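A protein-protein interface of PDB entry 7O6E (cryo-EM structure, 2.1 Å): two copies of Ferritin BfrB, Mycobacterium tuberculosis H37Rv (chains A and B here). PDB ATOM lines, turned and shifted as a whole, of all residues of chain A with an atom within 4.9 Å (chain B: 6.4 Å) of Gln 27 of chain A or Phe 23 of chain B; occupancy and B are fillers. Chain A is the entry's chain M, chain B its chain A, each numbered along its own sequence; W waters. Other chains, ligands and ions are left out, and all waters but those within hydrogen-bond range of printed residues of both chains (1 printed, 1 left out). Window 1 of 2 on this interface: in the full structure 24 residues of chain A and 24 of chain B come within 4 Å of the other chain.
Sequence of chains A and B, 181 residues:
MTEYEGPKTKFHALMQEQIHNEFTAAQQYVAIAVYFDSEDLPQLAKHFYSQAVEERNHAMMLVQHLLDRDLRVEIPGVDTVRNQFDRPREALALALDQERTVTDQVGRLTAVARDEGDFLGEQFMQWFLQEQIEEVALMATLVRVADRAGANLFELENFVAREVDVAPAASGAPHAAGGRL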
ATOM      1  N   PHE A  23       4.179  -1.922 -30.365  1.00  0.00           N
ATOM      2  CA  PHE A  23       4.361  -3.354 -30.168  1.00  0.00           C
ATOM      3  C   PHE A  23       3.109  -4.116 -30.589  1.00  0.00           C
ATOM      4  O   PHE A  23       3.194  -5.175 -31.216  1.00  0.00           O
ATOM      5  CB  PHE A  23       4.731  -3.668 -28.725  1.00  0.00           C
ATOM      6  CG  PHE A  23       6.183  -3.474 -28.399  1.00  0.00           C
ATOM      7  CD1 PHE A  23       7.172  -4.178 -29.057  1.00  0.00           C
ATOM      8  CD2 PHE A  23       6.555  -2.636 -27.381  1.00  0.00           C
ATOM      9  CE1 PHE A  23       8.482  -4.026 -28.718  1.00  0.00           C
ATOM     10  CE2 PHE A  23       7.879  -2.476 -27.053  1.00  0.00           C
ATOM     11  CZ  PHE A  23       8.837  -3.160 -27.718  1.00  0.00           C
ATOM     12  N   THR A  24       1.941  -3.568 -30.288  1.00  0.00           N
ATOM     13  CA  THR A  24       0.717  -4.211 -30.715  1.00  0.00           C
ATOM     14  C   THR A  24       0.613  -4.249 -32.231  1.00  0.00           C
ATOM     15  O   THR A  24       0.206  -5.254 -32.805  1.00  0.00           O
ATOM     16  CB  THR A  24      -0.487  -3.503 -30.109  1.00  0.00           C
ATOM     17  OG1 THR A  24      -0.484  -3.710 -28.701  1.00  0.00           O
ATOM     18  CG2 THR A  24      -1.717  -4.097 -30.625  1.00  0.00           C
ATOM     19  N   ALA A  25       1.000  -3.174 -32.888  1.00  0.00           N
ATOM     20  CA  ALA A  25       0.957  -3.133 -34.332  1.00  0.00           C
ATOM     21  C   ALA A  25       1.903  -4.155 -34.942  1.00  0.00           C
ATOM     22  O   ALA A  25       1.565  -4.807 -35.927  1.00  0.00           O
ATOM     23  CB  ALA A  25       1.303  -1.736 -34.819  1.00  0.00           C
ATOM     24  N   ALA A  26       3.094  -4.294 -34.379  1.00  0.00           N
ATOM     25  CA  ALA A  26       4.021  -5.291 -34.878  1.00  0.00           C
ATOM     26  C   ALA A  26       3.437  -6.687 -34.745  1.00  0.00           C
ATOM     27  O   ALA A  26       3.527  -7.503 -35.664  1.00  0.00           O
ATOM     28  CB  ALA A  26       5.346  -5.214 -34.143  1.00  0.00           C
ATOM     29  N   GLN A  27       2.815  -6.967 -33.617  1.00  0.00           N
ATOM     30  CA  GLN A  27       2.219  -8.273 -33.449  1.00  0.00           C
ATOM     31  C   GLN A  27       1.071  -8.499 -34.431  1.00  0.00           C
ATOM     32  O   GLN A  27       0.919  -9.595 -34.968  1.00  0.00           O
ATOM     33  CB  GLN A  27       1.774  -8.457 -32.010  1.00  0.00           C
ATOM     34  CG  GLN A  27       1.627  -9.910 -31.603  1.00  0.00           C
ATOM     35  CD  GLN A  27       2.948 -10.595 -31.370  1.00  0.00           C
ATOM     36  OE1 GLN A  27       3.990 -10.100 -31.743  1.00  0.00           O
ATOM     37  NE2 GLN A  27       2.899 -11.747 -30.755  1.00  0.00           N
ATOM     38  N   GLN A  28       0.269  -7.478 -34.690  1.00  0.00           N
ATOM     39  CA  GLN A  28      -0.804  -7.629 -35.658  1.00  0.00           C
ATOM     40  C   GLN A  28      -0.254  -7.888 -37.047  1.00  0.00           C
ATOM     41  O   GLN A  28      -0.829  -8.664 -37.813  1.00  0.00           O
ATOM     42  CB  GLN A  28      -1.702  -6.403 -35.661  1.00  0.00           C
ATOM     43  CG  GLN A  28      -2.859  -6.479 -36.636  1.00  0.00           C
ATOM     44  CD  GLN A  28      -3.847  -7.564 -36.332  1.00  0.00           C
ATOM     45  OE1 GLN A  28      -4.682  -7.427 -35.472  1.00  0.00           O
ATOM     46  NE2 GLN A  28      -3.754  -8.640 -37.044  1.00  0.00           N
ATOM     47  N   TYR A  29       0.852  -7.244 -37.392  1.00  0.00           N
ATOM     48  CA  TYR A  29       1.470  -7.500 -38.681  1.00  0.00           C
ATOM     49  C   TYR A  29       1.972  -8.933 -38.775  1.00  0.00           C
ATOM     50  O   TYR A  29       1.856  -9.566 -39.822  1.00  0.00           O
ATOM     51  CB  TYR A  29       2.607  -6.518 -38.947  1.00  0.00           C
ATOM     52  CG  TYR A  29       2.149  -5.239 -39.577  1.00  0.00           C
ATOM     53  CD1 TYR A  29       1.003  -5.207 -40.342  1.00  0.00           C
ATOM     54  CD2 TYR A  29       2.846  -4.046 -39.398  1.00  0.00           C
ATOM     55  CE1 TYR A  29       0.566  -4.059 -40.908  1.00  0.00           C
ATOM     56  CE2 TYR A  29       2.416  -2.876 -39.985  1.00  0.00           C
ATOM     57  CZ  TYR A  29       1.280  -2.892 -40.734  1.00  0.00           C
ATOM     58  OH  TYR A  29       0.808  -1.764 -41.309  1.00  0.00           O
ATOM     59  N   VAL A  30       2.537  -9.454 -37.695  1.00  0.00           N
ATOM     60  CA  VAL A  30       2.920 -10.858 -37.661  1.00  0.00           C
ATOM     61  C   VAL A  30       1.710 -11.753 -37.901  1.00  0.00           C
ATOM     62  O   VAL A  30       1.776 -12.728 -38.650  1.00  0.00           O
ATOM     63  CB  VAL A  30       3.591 -11.198 -36.316  1.00  0.00           C
ATOM     64  CG1 VAL A  30       3.723 -12.681 -36.156  1.00  0.00           C
ATOM     65  CG2 VAL A  30       4.914 -10.563 -36.200  1.00  0.00           C
ATOM     66  N   ALA A  31       0.603 -11.462 -37.233  1.00  0.00           N
ATOM     67  CA  ALA A  31      -0.588 -12.282 -37.416  1.00  0.00           C
ATOM     68  C   ALA A  31      -1.040 -12.264 -38.866  1.00  0.00           C
ATOM     69  O   ALA A  31      -1.411 -13.294 -39.428  1.00  0.00           O
ATOM     70  CB  ALA A  31      -1.710 -11.807 -36.508  1.00  0.00           C
ATOM     71  N   VAL A  78       1.044  -6.918 -24.787  1.00  0.00           N
ATOM     72  CA  VAL A  78       0.523  -6.733 -26.132  1.00  0.00           C
ATOM     73  C   VAL A  78      -0.909  -7.226 -26.159  1.00  0.00           C
ATOM     74  O   VAL A  78      -1.201  -8.310 -25.657  1.00  0.00           O
ATOM     75  CB  VAL A  78       1.356  -7.485 -27.189  1.00  0.00           C
ATOM     76  CG1 VAL A  78       0.675  -7.438 -28.545  1.00  0.00           C
ATOM     77  CG2 VAL A  78       2.736  -6.935 -27.307  1.00  0.00           C
ATOM     78  N   VAL A  81      -4.445  -9.869 -30.979  1.00  0.00           N
ATOM     79  CA  VAL A  81      -4.643  -9.286 -32.289  1.00  0.00           C
ATOM     80  C   VAL A  81      -5.595 -10.167 -33.059  1.00  0.00           C
ATOM     81  O   VAL A  81      -6.037 -11.203 -32.570  1.00  0.00           O
ATOM     82  CB  VAL A  81      -3.322  -9.101 -33.057  1.00  0.00           C
ATOM     83  CG1 VAL A  81      -2.453  -8.074 -32.377  1.00  0.00           C
ATOM     84  CG2 VAL A  81      -2.606 -10.417 -33.222  1.00  0.00           C
ATOM     85  N   GLN B  18       2.684 -22.728 -26.045  1.00  0.00           N
ATOM     86  CA  GLN B  18       4.102 -22.445 -26.048  1.00  0.00           C
ATOM     87  C   GLN B  18       4.413 -21.246 -26.904  1.00  0.00           C
ATOM     88  O   GLN B  18       5.359 -20.523 -26.629  1.00  0.00           O
ATOM     89  CB  GLN B  18       4.890 -23.640 -26.544  1.00  0.00           C
ATOM     90  CG  GLN B  18       6.345 -23.570 -26.162  1.00  0.00           C
ATOM     91  CD  GLN B  18       6.575 -23.262 -24.702  1.00  0.00           C
ATOM     92  OE1 GLN B  18       5.812 -23.637 -23.835  1.00  0.00           O
ATOM     93  NE2 GLN B  18       7.636 -22.581 -24.433  1.00  0.00           N
ATOM     94  N   ILE B  19       3.660 -21.053 -27.969  1.00  0.00           N
ATOM     95  CA  ILE B  19       3.855 -19.861 -28.771  1.00  0.00           C
ATOM     96  C   ILE B  19       3.544 -18.626 -27.946  1.00  0.00           C
ATOM     97  O   ILE B  19       4.295 -17.645 -27.956  1.00  0.00           O
ATOM     98  CB  ILE B  19       3.020 -19.931 -30.054  1.00  0.00           C
ATOM     99  CG1 ILE B  19       3.680 -20.878 -31.052  1.00  0.00           C
ATOM    100  CG2 ILE B  19       2.944 -18.603 -30.696  1.00  0.00           C
ATOM    101  CD1 ILE B  19       2.860 -21.156 -32.229  1.00  0.00           C
ATOM    102  N   HIS B  20       2.462 -18.677 -27.177  1.00  0.00           N
ATOM    103  CA  HIS B  20       2.208 -17.583 -26.252  1.00  0.00           C
ATOM    104  C   HIS B  20       3.374 -17.402 -25.272  1.00  0.00           C
ATOM    105  O   HIS B  20       3.841 -16.284 -25.055  1.00  0.00           O
ATOM    106  CB  HIS B  20       0.902 -17.777 -25.500  1.00  0.00           C
ATOM    107  CG  HIS B  20       0.720 -16.785 -24.404  1.00  0.00           C
ATOM    108  ND1 HIS B  20       0.293 -15.499 -24.635  1.00  0.00           N
ATOM    109  CD2 HIS B  20       0.992 -16.858 -23.082  1.00  0.00           C
ATOM    110  CE1 HIS B  20       0.257 -14.838 -23.498  1.00  0.00           C
ATOM    111  NE2 HIS B  20       0.675 -15.639 -22.540  1.00  0.00           N
ATOM    112  N   ASN B  21       3.874 -18.494 -24.706  1.00  0.00           N
ATOM    113  CA  ASN B  21       4.941 -18.404 -23.721  1.00  0.00           C
ATOM    114  C   ASN B  21       6.201 -17.812 -24.322  1.00  0.00           C
ATOM    115  O   ASN B  21       6.877 -17.020 -23.678  1.00  0.00           O
ATOM    116  CB  ASN B  21       5.266 -19.767 -23.118  1.00  0.00           C
ATOM    117  CG  ASN B  21       4.226 -20.236 -22.160  1.00  0.00           C
ATOM    118  OD1 ASN B  21       3.496 -19.453 -21.593  1.00  0.00           O
ATOM    119  ND2 ASN B  21       4.141 -21.527 -21.991  1.00  0.00           N
ATOM    120  N   GLU B  22       6.562 -18.228 -25.525  1.00  0.00           N
ATOM    121  CA  GLU B  22       7.774 -17.736 -26.153  1.00  0.00           C
ATOM    122  C   GLU B  22       7.674 -16.254 -26.469  1.00  0.00           C
ATOM    123  O   GLU B  22       8.621 -15.510 -26.233  1.00  0.00           O
ATOM    124  CB  GLU B  22       8.076 -18.509 -27.427  1.00  0.00           C
ATOM    125  CG  GLU B  22       8.639 -19.872 -27.269  1.00  0.00           C
ATOM    126  CD  GLU B  22       9.952 -19.905 -26.544  1.00  0.00           C
ATOM    127  OE1 GLU B  22      10.022 -20.531 -25.493  1.00  0.00           O
ATOM    128  OE2 GLU B  22      10.919 -19.324 -27.052  1.00  0.00           O
ATOM    129  N   PHE B  23       6.554 -15.805 -27.029  1.00  0.00           N
ATOM    130  CA  PHE B  23       6.435 -14.375 -27.273  1.00  0.00           C
ATOM    131  C   PHE B  23       6.521 -13.598 -25.963  1.00  0.00           C
ATOM    132  O   PHE B  23       7.165 -12.548 -25.892  1.00  0.00           O
ATOM    133  CB  PHE B  23       5.146 -14.049 -28.015  1.00  0.00           C
ATOM    134  CG  PHE B  23       5.213 -14.262 -29.499  1.00  0.00           C
ATOM    135  CD1 PHE B  23       6.120 -13.581 -30.287  1.00  0.00           C
ATOM    136  CD2 PHE B  23       4.317 -15.094 -30.118  1.00  0.00           C
ATOM    137  CE1 PHE B  23       6.137 -13.749 -31.638  1.00  0.00           C
ATOM    138  CE2 PHE B  23       4.348 -15.270 -31.479  1.00  0.00           C
ATOM    139  CZ  PHE B  23       5.253 -14.609 -32.235  1.00  0.00           C
ATOM    140  N   THR B  24       5.914 -14.125 -24.910  1.00  0.00           N
ATOM    141  CA  THR B  24       6.011 -13.468 -23.624  1.00  0.00           C
ATOM    142  C   THR B  24       7.446 -13.447 -23.123  1.00  0.00           C
ATOM    143  O   THR B  24       7.907 -12.442 -22.591  1.00  0.00           O
ATOM    144  CB  THR B  24       5.098 -14.150 -22.616  1.00  0.00           C
ATOM    145  OG1 THR B  24       3.744 -13.927 -22.993  1.00  0.00           O
ATOM    146  CG2 THR B  24       5.279 -13.543 -21.299  1.00  0.00           C
ATOM    147  N   ALA B  25       8.166 -14.534 -23.310  1.00  0.00           N
ATOM    148  CA  ALA B  25       9.546 -14.593 -22.886  1.00  0.00           C
ATOM    149  C   ALA B  25      10.401 -13.592 -23.648  1.00  0.00           C
ATOM    150  O   ALA B  25      11.271 -12.947 -23.070  1.00  0.00           O
ATOM    151  CB  ALA B  25      10.086 -15.999 -23.075  1.00  0.00           C
ATOM    152  N   ALA B  26      10.175 -13.465 -24.948  1.00  0.00           N
ATOM    153  CA  ALA B  26      10.916 -12.488 -25.721  1.00  0.00           C
ATOM    154  C   ALA B  26      10.655 -11.082 -25.210  1.00  0.00           C
ATOM    155  O   ALA B  26      11.578 -10.278 -25.062  1.00  0.00           O
ATOM    156  CB  ALA B  26      10.557 -12.577 -27.192  1.00  0.00           C
ATOM    157  N   GLN B  27       9.407 -10.779 -24.912  1.00  0.00           N
ATOM    158  CA  GLN B  27       9.108  -9.462 -24.397  1.00  0.00           C
ATOM    159  C   GLN B  27       9.754  -9.230 -23.032  1.00  0.00           C
ATOM    160  O   GLN B  27      10.249  -8.138 -22.757  1.00  0.00           O
ATOM    161  CB  GLN B  27       7.605  -9.254 -24.351  1.00  0.00           C
ATOM    162  CG  GLN B  27       7.196  -7.794 -24.334  1.00  0.00           C
ATOM    163  CD  GLN B  27       7.331  -7.128 -25.677  1.00  0.00           C
ATOM    164  OE1 GLN B  27       7.959  -7.642 -26.578  1.00  0.00           O
ATOM    165  NE2 GLN B  27       6.743  -5.968 -25.806  1.00  0.00           N
ATOM    166  N   GLN B  28       9.777 -10.241 -22.179  1.00  0.00           N
ATOM    167  CA  GLN B  28      10.428 -10.085 -20.890  1.00  0.00           C
ATOM    168  C   GLN B  28      11.917  -9.851 -21.055  1.00  0.00           C
ATOM    169  O   GLN B  28      12.515  -9.075 -20.307  1.00  0.00           O
ATOM    170  CB  GLN B  28      10.175 -11.297 -20.009  1.00  0.00           C
ATOM    171  CG  GLN B  28      10.810 -11.215 -18.636  1.00  0.00           C
ATOM    172  CD  GLN B  28      10.272 -10.111 -17.777  1.00  0.00           C
ATOM    173  OE1 GLN B  28       9.220 -10.225 -17.198  1.00  0.00           O
ATOM    174  NE2 GLN B  28      11.000  -9.045 -17.690  1.00  0.00           N
ATOM    175  N   GLU B  55      14.685 -15.419 -28.739  1.00  0.00           N
ATOM    176  CA  GLU B  55      13.421 -15.962 -28.262  1.00  0.00           C
ATOM    177  C   GLU B  55      12.320 -15.741 -29.287  1.00  0.00           C
ATOM    178  O   GLU B  55      11.455 -16.599 -29.483  1.00  0.00           O
ATOM    179  CB  GLU B  55      13.008 -15.327 -26.944  1.00  0.00           C
ATOM    180  CG  GLU B  55      13.457 -16.023 -25.681  1.00  0.00           C
ATOM    181  CD  GLU B  55      13.583 -17.527 -25.777  1.00  0.00           C
ATOM    182  OE1 GLU B  55      12.598 -18.225 -25.534  1.00  0.00           O
ATOM    183  OE2 GLU B  55      14.676 -18.014 -26.126  1.00  0.00           O
ATOM    184  N   ARG B  56      12.321 -14.577 -29.919  1.00  0.00           N
ATOM    185  CA  ARG B  56      11.360 -14.320 -30.973  1.00  0.00           C
ATOM    186  C   ARG B  56      11.504 -15.338 -32.090  1.00  0.00           C
ATOM    187  O   ARG B  56      10.511 -15.849 -32.606  1.00  0.00           O
ATOM    188  CB  ARG B  56      11.538 -12.911 -31.514  1.00  0.00           C
ATOM    189  CG  ARG B  56      10.511 -12.541 -32.544  1.00  0.00           C
ATOM    190  CD  ARG B  56      10.889 -11.311 -33.244  1.00  0.00           C
ATOM    191  NE  ARG B  56       9.767 -10.679 -33.906  1.00  0.00           N
ATOM    192  CZ  ARG B  56       9.517 -10.805 -35.200  1.00  0.00           C
ATOM    193  NH1 ARG B  56      10.295 -11.553 -35.947  1.00  0.00           N
ATOM    194  NH2 ARG B  56       8.493 -10.202 -35.742  1.00  0.00           N
ATOM    195  N   ALA B  59       9.824 -18.580 -31.120  1.00  0.00           N
ATOM    196  CA  ALA B  59       8.391 -18.518 -31.286  1.00  0.00           C
ATOM    197  C   ALA B  59       8.028 -18.672 -32.748  1.00  0.00           C
ATOM    198  O   ALA B  59       7.093 -19.380 -33.075  1.00  0.00           O
ATOM    199  CB  ALA B  59       7.836 -17.217 -30.734  1.00  0.00           C
ATOM    200  N   MET B  60       8.767 -18.014 -33.619  1.00  0.00           N
ATOM    201  CA  MET B  60       8.525 -18.170 -35.035  1.00  0.00           C
ATOM    202  C   MET B  60       8.721 -19.606 -35.503  1.00  0.00           C
ATOM    203  O   MET B  60       8.025 -20.060 -36.403  1.00  0.00           O
ATOM    204  CB  MET B  60       9.429 -17.244 -35.808  1.00  0.00           C
ATOM    205  CG  MET B  60       9.061 -15.829 -35.646  1.00  0.00           C
ATOM    206  SD  MET B  60       7.332 -15.506 -35.306  1.00  0.00           S
ATOM    207  CE  MET B  60       6.780 -15.114 -36.949  1.00  0.00           C
ATOM    208  N   VAL B  63       5.601 -21.412 -34.597  1.00  0.00           N
ATOM    209  CA  VAL B  63       4.609 -21.003 -35.577  1.00  0.00           C
ATOM    210  C   VAL B  63       4.804 -21.774 -36.874  1.00  0.00           C
ATOM    211  O   VAL B  63       3.862 -22.343 -37.421  1.00  0.00           O
ATOM    212  CB  VAL B  63       4.685 -19.486 -35.815  1.00  0.00           C
ATOM    213  CG1 VAL B  63       3.956 -19.126 -37.074  1.00  0.00           C
ATOM    214  CG2 VAL B  63       4.137 -18.752 -34.658  1.00  0.00           C
ATOM    215  N   GLU B  74      -2.599 -19.329 -34.058  1.00  0.00           N
ATOM    216  CA  GLU B  74      -2.993 -17.919 -33.835  1.00  0.00           C
ATOM    217  C   GLU B  74      -1.836 -17.156 -33.200  1.00  0.00           C
ATOM    218  O   GLU B  74      -1.169 -17.730 -32.334  1.00  0.00           O
ATOM    219  CB  GLU B  74      -4.138 -17.880 -32.832  1.00  0.00           C
ATOM    220  CG  GLU B  74      -5.504 -17.931 -33.482  1.00  0.00           C
ATOM    221  CD  GLU B  74      -6.162 -19.298 -33.448  1.00  0.00           C
ATOM    222  OE1 GLU B  74      -5.495 -20.262 -33.024  1.00  0.00           O
ATOM    223  OE2 GLU B  74      -7.339 -19.396 -33.846  1.00  0.00           O
ATOM    224  N   ILE B  75      -1.572 -15.939 -33.649  1.00  0.00           N
ATOM    225  CA  ILE B  75      -0.600 -15.089 -32.995  1.00  0.00           C
ATOM    226  C   ILE B  75      -1.244 -14.480 -31.756  1.00  0.00           C
ATOM    227  O   ILE B  75      -2.278 -13.816 -31.855  1.00  0.00           O
ATOM    228  CB  ILE B  75      -0.067 -14.049 -33.977  1.00  0.00           C
ATOM    229  CG1 ILE B  75       0.574 -14.771 -35.161  1.00  0.00           C
ATOM    230  CG2 ILE B  75       0.926 -13.174 -33.312  1.00  0.00           C
ATOM    231  CD1 ILE B  75       1.646 -15.734 -34.780  1.00  0.00           C
ATOM    232  N   PRO B  76      -0.711 -14.730 -30.577  1.00  0.00           N
ATOM    233  CA  PRO B  76      -1.396 -14.303 -29.356  1.00  0.00           C
ATOM    234  C   PRO B  76      -1.080 -12.875 -28.939  1.00  0.00           C
ATOM    235  O   PRO B  76      -0.229 -12.221 -29.528  1.00  0.00           O
ATOM    236  CB  PRO B  76      -0.881 -15.303 -28.321  1.00  0.00           C
ATOM    237  CG  PRO B  76       0.495 -15.538 -28.736  1.00  0.00           C
ATOM    238  CD  PRO B  76       0.522 -15.473 -30.263  1.00  0.00           C
ATOM    239  N   GLY B  77      -1.743 -12.395 -27.901  1.00  0.00           N
ATOM    240  CA  GLY B  77      -1.252 -11.254 -27.168  1.00  0.00           C
ATOM    241  C   GLY B  77      -0.005 -11.620 -26.379  1.00  0.00           C
ATOM    242  O   GLY B  77       0.571 -12.688 -26.523  1.00  0.00           O
ATOM    243  N   VAL B  78       0.423 -10.697 -25.541  1.00  0.00           N
ATOM    244  CA  VAL B  78       1.580 -10.890 -24.680  1.00  0.00           C
ATOM    245  C   VAL B  78       1.234 -10.375 -23.298  1.00  0.00           C
ATOM    246  O   VAL B  78       0.690  -9.281 -23.162  1.00  0.00           O
ATOM    247  CB  VAL B  78       2.831 -10.163 -25.212  1.00  0.00           C
ATOM    248  CG1 VAL B  78       3.957 -10.216 -24.196  1.00  0.00           C
ATOM    249  CG2 VAL B  78       3.301 -10.736 -26.505  1.00  0.00           C
HETATM  250  O   HOH W   1       7.456  -9.786 -31.964  1.00  0.00           O
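NE2 of Gln 27 of chain A lies within hydrogen-bond range of O of Pro 76 of chain B. The backbone NH of Val 78 of chain B is in hydrogen-bond range of the backbone carbonyl oxygen of Val 78 of chain A.
The backbone carbonyl oxygen (O) of Gly 77 of chain B is in hydrogen-bond range of a ring nitrogen (ND1) of His 20 of chain B (3.4 Å).
Among the printed residues, merely in contact across the chains: Phe 23 of chain A with Gln 27 of chain B, Gln 27 of chain A with Phe 23 of chain B, Gln 27 of chain A with Ile 75 of chain B, Val 30 of chain A with Arg 56 of chain B, Val 30 of chain A with Met 60 of chain B, Val 30 of chain A with Ile 75 of chain B, Ala 31 of chain A with Ile 75 of chain B, Val 78 of chain A with Gly 77 of chain B and Val 81 of chain A with Ile 75 of chain B.
Gln 27 of chain A touches three residues of chain B. Of the printed residues of chain A, Val 78 of chain B touches Val 78 (2.9 Å). Of the printed residues of chain B, Phe 23 of chain A touches Gln 27 (3.6 Å). Glu 74 of chain B touches none of the printed residues of chain A. The nearest residue of chain B that does not touch Gln 27 of chain A is Val 78 of chain B (4.4 Å).
Hydrophobic or aromatic side chains of chain A within 4 Å of the printed part of chain B: Phe 23, Val 30, Ala 31, Val 78 and Val 81. Of the 21 printed residues of chain B, 8 touch a printed residue of chain A. Hydrophobic or aromatic side chains of chain B within 4 Å of the printed part of chain A: Phe 23, Met 60, Ile 75 and Val 78. Among the printed residues, 11 pairs touch across the chains.
Phe 23 of chain A touches Gln 27 of chain B, and with the chains exchanged Gln 27 of chain A touches Phe 23 of chain B. Val 78 of chain B touches its own counterpart, Val 78 of chain A. Positions printed for both chains: 23, 24, 25, 26, 27, 28 and 78.
Water W1 bridges the guanidinium group (NE) of Arg 56 of chain B and the side-chain amide oxygen (OE1) of Gln 27 of chain A.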
